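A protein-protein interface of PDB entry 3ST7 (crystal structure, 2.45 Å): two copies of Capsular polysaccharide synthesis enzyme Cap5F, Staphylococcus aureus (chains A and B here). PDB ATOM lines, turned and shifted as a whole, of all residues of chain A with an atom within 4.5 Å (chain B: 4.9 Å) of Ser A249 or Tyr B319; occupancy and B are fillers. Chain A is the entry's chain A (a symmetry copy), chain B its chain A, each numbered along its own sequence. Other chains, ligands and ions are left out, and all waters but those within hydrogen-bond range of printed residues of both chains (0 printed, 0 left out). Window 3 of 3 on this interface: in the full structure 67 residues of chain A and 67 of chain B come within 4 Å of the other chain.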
ATOM      1  N   ARG A 219     -24.488 -13.455 -28.458  1.00  0.00           N
ATOM      2  CA  ARG A 219     -23.873 -13.960 -27.251  1.00  0.00           C
ATOM      3  C   ARG A 219     -24.094 -15.463 -27.173  1.00  0.00           C
ATOM      4  O   ARG A 219     -23.164 -16.208 -26.969  1.00  0.00           O
ATOM      5  CB  ARG A 219     -24.540 -13.310 -26.058  1.00  0.00           C
ATOM      6  CG  ARG A 219     -23.765 -13.352 -24.784  1.00  0.00           C
ATOM      7  CD  ARG A 219     -23.221 -11.965 -24.533  1.00  0.00           C
ATOM      8  NE  ARG A 219     -23.559 -11.563 -23.196  1.00  0.00           N
ATOM      9  CZ  ARG A 219     -22.962 -10.599 -22.515  1.00  0.00           C
ATOM     10  NH1 ARG A 219     -21.948  -9.933 -23.019  1.00  0.00           N
ATOM     11  NH2 ARG A 219     -23.385 -10.341 -21.287  1.00  0.00           N
ATOM     12  N   SER A 245     -23.021  -3.350 -15.910  1.00  0.00           N
ATOM     13  CA  SER A 245     -21.640  -3.589 -15.537  1.00  0.00           C
ATOM     14  C   SER A 245     -21.404  -4.959 -14.898  1.00  0.00           C
ATOM     15  O   SER A 245     -20.259  -5.380 -14.755  1.00  0.00           O
ATOM     16  CB  SER A 245     -21.128  -2.455 -14.645  1.00  0.00           C
ATOM     17  OG  SER A 245     -21.776  -2.466 -13.386  1.00  0.00           O
ATOM     18  N   THR A 246     -22.485  -5.653 -14.532  1.00  0.00           N
ATOM     19  CA  THR A 246     -22.418  -7.020 -14.012  1.00  0.00           C
ATOM     20  C   THR A 246     -22.578  -8.061 -15.117  1.00  0.00           C
ATOM     21  O   THR A 246     -22.617  -9.271 -14.841  1.00  0.00           O
ATOM     22  CB  THR A 246     -23.559  -7.307 -13.032  1.00  0.00           C
ATOM     23  OG1 THR A 246     -24.815  -7.029 -13.672  1.00  0.00           O
ATOM     24  CG2 THR A 246     -23.416  -6.488 -11.739  1.00  0.00           C
ATOM     25  N   ASP A 247     -22.695  -7.610 -16.358  1.00  0.00           N
ATOM     26  CA  ASP A 247     -23.052  -8.516 -17.429  1.00  0.00           C
ATOM     27  C   ASP A 247     -22.060  -8.526 -18.606  1.00  0.00           C
ATOM     28  O   ASP A 247     -22.438  -8.750 -19.746  1.00  0.00           O
ATOM     29  CB  ASP A 247     -24.491  -8.222 -17.856  1.00  0.00           C
ATOM     30  CG  ASP A 247     -25.093  -9.304 -18.758  1.00  0.00           C
ATOM     31  OD1 ASP A 247     -24.811 -10.545 -18.603  1.00  0.00           O
ATOM     32  OD2 ASP A 247     -25.873  -8.872 -19.647  1.00  0.00           O
ATOM     33  N   PHE A 248     -20.778  -8.317 -18.322  1.00  0.00           N
ATOM     34  CA  PHE A 248     -19.771  -8.282 -19.373  1.00  0.00           C
ATOM     35  C   PHE A 248     -19.333  -9.671 -19.804  1.00  0.00           C
ATOM     36  O   PHE A 248     -18.720  -9.828 -20.857  1.00  0.00           O
ATOM     37  CB  PHE A 248     -18.539  -7.499 -18.913  1.00  0.00           C
ATOM     38  CG  PHE A 248     -18.775  -6.009 -18.695  1.00  0.00           C
ATOM     39  CD1 PHE A 248     -19.984  -5.407 -19.020  1.00  0.00           C
ATOM     40  CD2 PHE A 248     -17.751  -5.214 -18.190  1.00  0.00           C
ATOM     41  CE1 PHE A 248     -20.175  -4.045 -18.839  1.00  0.00           C
ATOM     42  CE2 PHE A 248     -17.932  -3.854 -17.991  1.00  0.00           C
ATOM     43  CZ  PHE A 248     -19.147  -3.260 -18.327  1.00  0.00           C
ATOM     44  N   SER A 249     -19.628 -10.677 -18.987  1.00  0.00           N
ATOM     45  CA  SER A 249     -19.200 -12.043 -19.248  1.00  0.00           C
ATOM     46  C   SER A 249     -20.359 -12.975 -19.562  1.00  0.00           C
ATOM     47  O   SER A 249     -21.489 -12.693 -19.195  1.00  0.00           O
ATOM     48  CB  SER A 249     -18.430 -12.601 -18.051  1.00  0.00           C
ATOM     49  OG  SER A 249     -19.302 -12.844 -16.942  1.00  0.00           O
ATOM     50  N   TYR A 250     -20.056 -14.093 -20.231  1.00  0.00           N
ATOM     51  CA  TYR A 250     -21.045 -15.123 -20.513  1.00  0.00           C
ATOM     52  C   TYR A 250     -20.361 -16.485 -20.563  1.00  0.00           C
ATOM     53  O   TYR A 250     -19.241 -16.589 -21.043  1.00  0.00           O
ATOM     54  CB  TYR A 250     -21.850 -14.833 -21.793  1.00  0.00           C
ATOM     55  CG  TYR A 250     -21.045 -14.654 -23.054  1.00  0.00           C
ATOM     56  CD1 TYR A 250     -20.474 -13.424 -23.356  1.00  0.00           C
ATOM     57  CD2 TYR A 250     -20.868 -15.703 -23.964  1.00  0.00           C
ATOM     58  CE1 TYR A 250     -19.721 -13.222 -24.514  1.00  0.00           C
ATOM     59  CE2 TYR A 250     -20.100 -15.516 -25.148  1.00  0.00           C
ATOM     60  CZ  TYR A 250     -19.536 -14.263 -25.405  1.00  0.00           C
ATOM     61  OH  TYR A 250     -18.790 -14.019 -26.537  1.00  0.00           O
ATOM     62  N   GLY B 304      -6.860 -15.733 -13.085  1.00  0.00           N
ATOM     63  CA  GLY B 304      -6.594 -14.347 -12.780  1.00  0.00           C
ATOM     64  C   GLY B 304      -7.865 -13.542 -12.748  1.00  0.00           C
ATOM     65  O   GLY B 304      -8.950 -14.082 -12.501  1.00  0.00           O
ATOM     66  N   VAL B 305      -7.735 -12.245 -13.009  1.00  0.00           N
ATOM     67  CA  VAL B 305      -8.863 -11.344 -12.914  1.00  0.00           C
ATOM     68  C   VAL B 305      -8.818 -10.361 -14.070  1.00  0.00           C
ATOM     69  O   VAL B 305      -7.742  -9.921 -14.468  1.00  0.00           O
ATOM     70  CB  VAL B 305      -8.889 -10.595 -11.540  1.00  0.00           C
ATOM     71  CG1 VAL B 305      -7.610  -9.850 -11.296  1.00  0.00           C
ATOM     72  CG2 VAL B 305     -10.053  -9.622 -11.462  1.00  0.00           C
ATOM     73  N   ILE B 306      -9.992 -10.036 -14.602  1.00  0.00           N
ATOM     74  CA  ILE B 306     -10.124  -8.999 -15.609  1.00  0.00           C
ATOM     75  C   ILE B 306     -10.838  -7.835 -14.950  1.00  0.00           C
ATOM     76  O   ILE B 306     -11.904  -8.012 -14.372  1.00  0.00           O
ATOM     77  CB  ILE B 306     -10.902  -9.502 -16.863  1.00  0.00           C
ATOM     78  CG1 ILE B 306     -10.237 -10.750 -17.467  1.00  0.00           C
ATOM     79  CG2 ILE B 306     -11.014  -8.381 -17.918  1.00  0.00           C
ATOM     80  CD1 ILE B 306     -11.113 -11.492 -18.465  1.00  0.00           C
ATOM     81  N   PHE B 308     -12.314  -3.649 -14.783  1.00  0.00           N
ATOM     82  CA  PHE B 308     -12.928  -2.571 -15.551  1.00  0.00           C
ATOM     83  C   PHE B 308     -13.162  -1.389 -14.671  1.00  0.00           C
ATOM     84  O   PHE B 308     -13.445  -1.537 -13.492  1.00  0.00           O
ATOM     85  CB  PHE B 308     -14.291  -2.987 -16.095  1.00  0.00           C
ATOM     86  CG  PHE B 308     -14.240  -4.124 -17.035  1.00  0.00           C
ATOM     87  CD1 PHE B 308     -14.052  -3.909 -18.397  1.00  0.00           C
ATOM     88  CD2 PHE B 308     -14.385  -5.426 -16.579  1.00  0.00           C
ATOM     89  CE1 PHE B 308     -14.006  -4.987 -19.279  1.00  0.00           C
ATOM     90  CE2 PHE B 308     -14.348  -6.505 -17.460  1.00  0.00           C
ATOM     91  CZ  PHE B 308     -14.148  -6.288 -18.800  1.00  0.00           C
ATOM     92  N   ILE B 317     -14.666  -2.728 -11.320  1.00  0.00           N
ATOM     93  CA  ILE B 317     -15.438  -3.963 -11.443  1.00  0.00           C
ATOM     94  C   ILE B 317     -14.496  -5.114 -11.807  1.00  0.00           C
ATOM     95  O   ILE B 317     -13.735  -5.011 -12.769  1.00  0.00           O
ATOM     96  CB  ILE B 317     -16.531  -3.841 -12.530  1.00  0.00           C
ATOM     97  CG1 ILE B 317     -17.374  -2.590 -12.300  1.00  0.00           C
ATOM     98  CG2 ILE B 317     -17.431  -5.075 -12.552  1.00  0.00           C
ATOM     99  CD1 ILE B 317     -17.742  -1.870 -13.588  1.00  0.00           C
ATOM    100  N   GLU B 318     -14.568  -6.211 -11.052  1.00  0.00           N
ATOM    101  CA  GLU B 318     -13.635  -7.322 -11.193  1.00  0.00           C
ATOM    102  C   GLU B 318     -14.324  -8.580 -11.659  1.00  0.00           C
ATOM    103  O   GLU B 318     -15.359  -8.973 -11.098  1.00  0.00           O
ATOM    104  CB  GLU B 318     -12.935  -7.607  -9.865  1.00  0.00           C
ATOM    105  CG  GLU B 318     -11.989  -6.513  -9.411  1.00  0.00           C
ATOM    106  CD  GLU B 318     -11.260  -6.853  -8.116  1.00  0.00           C
ATOM    107  OE1 GLU B 318     -11.881  -7.445  -7.198  1.00  0.00           O
ATOM    108  OE2 GLU B 318     -10.062  -6.512  -8.013  1.00  0.00           O
ATOM    109  N   TYR B 319     -13.743  -9.213 -12.684  1.00  0.00           N
ATOM    110  CA  TYR B 319     -14.182 -10.528 -13.130  1.00  0.00           C
ATOM    111  C   TYR B 319     -13.115 -11.577 -12.861  1.00  0.00           C
ATOM    112  O   TYR B 319     -12.077 -11.610 -13.535  1.00  0.00           O
ATOM    113  CB  TYR B 319     -14.548 -10.529 -14.614  1.00  0.00           C
ATOM    114  CG  TYR B 319     -15.861  -9.855 -14.907  1.00  0.00           C
ATOM    115  CD1 TYR B 319     -16.975 -10.605 -15.272  1.00  0.00           C
ATOM    116  CD2 TYR B 319     -15.991  -8.456 -14.810  1.00  0.00           C
ATOM    117  CE1 TYR B 319     -18.187  -9.992 -15.548  1.00  0.00           C
ATOM    118  CE2 TYR B 319     -17.194  -7.827 -15.070  1.00  0.00           C
ATOM    119  CZ  TYR B 319     -18.288  -8.595 -15.448  1.00  0.00           C
ATOM    120  OH  TYR B 319     -19.494  -7.976 -15.712  1.00  0.00           O
ATOM    121  N   TYR B 320     -13.382 -12.428 -11.873  1.00  0.00           N
ATOM    122  CA  TYR B 320     -12.477 -13.520 -11.539  1.00  0.00           C
ATOM    123  C   TYR B 320     -12.693 -14.664 -12.482  1.00  0.00           C
ATOM    124  O   TYR B 320     -13.826 -15.110 -12.708  1.00  0.00           O
ATOM    125  CB  TYR B 320     -12.601 -13.932 -10.066  1.00  0.00           C
ATOM    126  CG  TYR B 320     -12.014 -12.860  -9.202  1.00  0.00           C
ATOM    127  CD1 TYR B 320     -12.806 -11.835  -8.705  1.00  0.00           C
ATOM    128  CD2 TYR B 320     -10.646 -12.826  -8.942  1.00  0.00           C
ATOM    129  CE1 TYR B 320     -12.261 -10.816  -7.929  1.00  0.00           C
ATOM    130  CE2 TYR B 320     -10.080 -11.809  -8.176  1.00  0.00           C
ATOM    131  CZ  TYR B 320     -10.894 -10.801  -7.669  1.00  0.00           C
ATOM    132  OH  TYR B 320     -10.343  -9.782  -6.905  1.00  0.00           O
ATOM    133  N   VAL B 321     -11.594 -15.154 -13.034  1.00  0.00           N
ATOM    134  CA  VAL B 321     -11.705 -15.972 -14.223  1.00  0.00           C
ATOM    135  C   VAL B 321     -10.547 -16.983 -14.339  1.00  0.00           C
ATOM    136  O   VAL B 321      -9.415 -16.696 -13.908  1.00  0.00           O
ATOM    137  CB  VAL B 321     -11.877 -14.984 -15.419  1.00  0.00           C
ATOM    138  CG1 VAL B 321     -10.558 -14.661 -16.115  1.00  0.00           C
ATOM    139  CG2 VAL B 321     -13.007 -15.404 -16.310  1.00  0.00           C
ATOM    140  N   GLU B 327     -15.301 -19.111 -19.886  1.00  0.00           N
ATOM    141  CA  GLU B 327     -16.256 -18.023 -19.997  1.00  0.00           C
ATOM    142  C   GLU B 327     -15.641 -16.782 -20.641  1.00  0.00           C
ATOM    143  O   GLU B 327     -14.497 -16.415 -20.366  1.00  0.00           O
ATOM    144  CB  GLU B 327     -16.896 -17.722 -18.630  1.00  0.00           C
ATOM    145  CG  GLU B 327     -15.969 -17.110 -17.620  1.00  0.00           C
ATOM    146  CD  GLU B 327     -16.518 -17.166 -16.197  1.00  0.00           C
ATOM    147  OE1 GLU B 327     -17.734 -16.943 -15.993  1.00  0.00           O
ATOM    148  OE2 GLU B 327     -15.719 -17.429 -15.272  1.00  0.00           O
ATOM    149  N   VAL B 328     -16.404 -16.166 -21.535  1.00  0.00           N
ATOM    150  CA  VAL B 328     -15.936 -15.010 -22.284  1.00  0.00           C
ATOM    151  C   VAL B 328     -16.251 -13.741 -21.499  1.00  0.00           C
ATOM    152  O   VAL B 328     -17.323 -13.620 -20.914  1.00  0.00           O
ATOM    153  CB  VAL B 328     -16.617 -14.945 -23.649  1.00  0.00           C
ATOM    154  CG1 VAL B 328     -16.212 -13.650 -24.422  1.00  0.00           C
ATOM    155  CG2 VAL B 328     -16.321 -16.201 -24.468  1.00  0.00           C
ATOM    156  N   VAL B 329     -15.306 -12.817 -21.451  1.00  0.00           N
ATOM    157  CA  VAL B 329     -15.567 -11.498 -20.922  1.00  0.00           C
ATOM    158  C   VAL B 329     -15.477 -10.506 -22.068  1.00  0.00           C
ATOM    159  O   VAL B 329     -14.410 -10.347 -22.661  1.00  0.00           O
ATOM    160  CB  VAL B 329     -14.575 -11.137 -19.821  1.00  0.00           C
ATOM    161  CG1 VAL B 329     -14.959  -9.820 -19.180  1.00  0.00           C
ATOM    162  CG2 VAL B 329     -14.536 -12.246 -18.749  1.00  0.00           C
ATOM    163  N   ASP B 330     -16.593  -9.870 -22.421  1.00  0.00           N
ATOM    164  CA  ASP B 330     -16.543  -8.786 -23.412  1.00  0.00           C
ATOM    165  C   ASP B 330     -15.808  -7.611 -22.814  1.00  0.00           C
ATOM    166  O   ASP B 330     -15.861  -7.409 -21.602  1.00  0.00           O
ATOM    167  CB  ASP B 330     -17.921  -8.304 -23.808  1.00  0.00           C
ATOM    168  CG  ASP B 330     -18.615  -9.230 -24.739  1.00  0.00           C
ATOM    169  OD1 ASP B 330     -18.084  -9.635 -25.804  1.00  0.00           O
ATOM    170  OD2 ASP B 330     -19.757  -9.530 -24.404  1.00  0.00           O
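The backbone carbonyl oxygen (O) of Ser A245 lies within hydrogen-bond range of the side-chain hydroxyl (OH) of Tyr B319, 2.9 Å away.
OH of Tyr B319 sits close to O of Thr A246.
The side-chain hydroxyl of Tyr B319 lies within hydrogen-bond range of the backbone NH of Asp A247 (3.3 Å).
The backbone NH (N) of Phe A248 lies within hydrogen-bond range of the side-chain hydroxyl (OH) of Tyr B319, at 2.9 Å.
The backbone NH (N) of Tyr A250 lies within hydrogen-bond range of the backbone carbonyl oxygen (O) of Val B328, 2.9 Å away.
The guanidinium group (NH1) of Arg A219 lies within salt-bridge range of the side-chain carboxylate (OD2) of Asp B330, at 2.6 Å.
The backbone NH (N) of Asp B330 is in hydrogen-bond range of the backbone carbonyl oxygen (O) of Phe A248, at 2.6 Å.
The backbone NH (N) of Tyr B319 is in hydrogen-bond range of the backbone carbonyl oxygen (O) of Ile B306, 2.8 Å away.
O of Phe B308 is in hydrogen-bond range of N of Ile B317.
OD1 of Asp A247 lies within salt-bridge range of NH2 of Arg A219, 3.0 Å away.
Among the printed residues, merely in contact across the chains: Ser A245 with Ile B317, Phe A248 with Phe B308, Phe A248 with Val B329, Ser A249 with Tyr B319, Ser A249 with Val B328, Ser A249 with Val B329, Tyr A250 with Glu B327 and Tyr A250 with Asp B330.
Of chain B, only Tyr B319, Val B328 and Val B329 come within 4 Å of Ser A249.
Gly B304 touches none of the printed residues of chain A.
Tyr B319 touches just these residues of chain A: Ser A245 (2.9 Å), Thr A246 (3.1 Å), Asp A247 (3.3 Å), Phe A248 (2.9 Å) and Ser A249 (3.4 Å).
Printed residues of chain A within 4 Å of Glu B327: Tyr A250 (3.5 Å).
Of the printed residues of chain A, Val B329 touches Phe A248 (3.5 Å) and Ser A249 (3.97 Å).
The nearest printed residue of chain A that does not touch Phe B308 is Ser A245 (6.2 Å).
Hydrophobic or aromatic side chains of chain A within 4 Å of the printed part of chain B: Phe A248 and Tyr A250.
Of the 13 printed residues of chain B, 7 touch a printed residue of chain A.
Among the printed residues, 15 pairs touch across the chains.
No position is printed for both chains.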
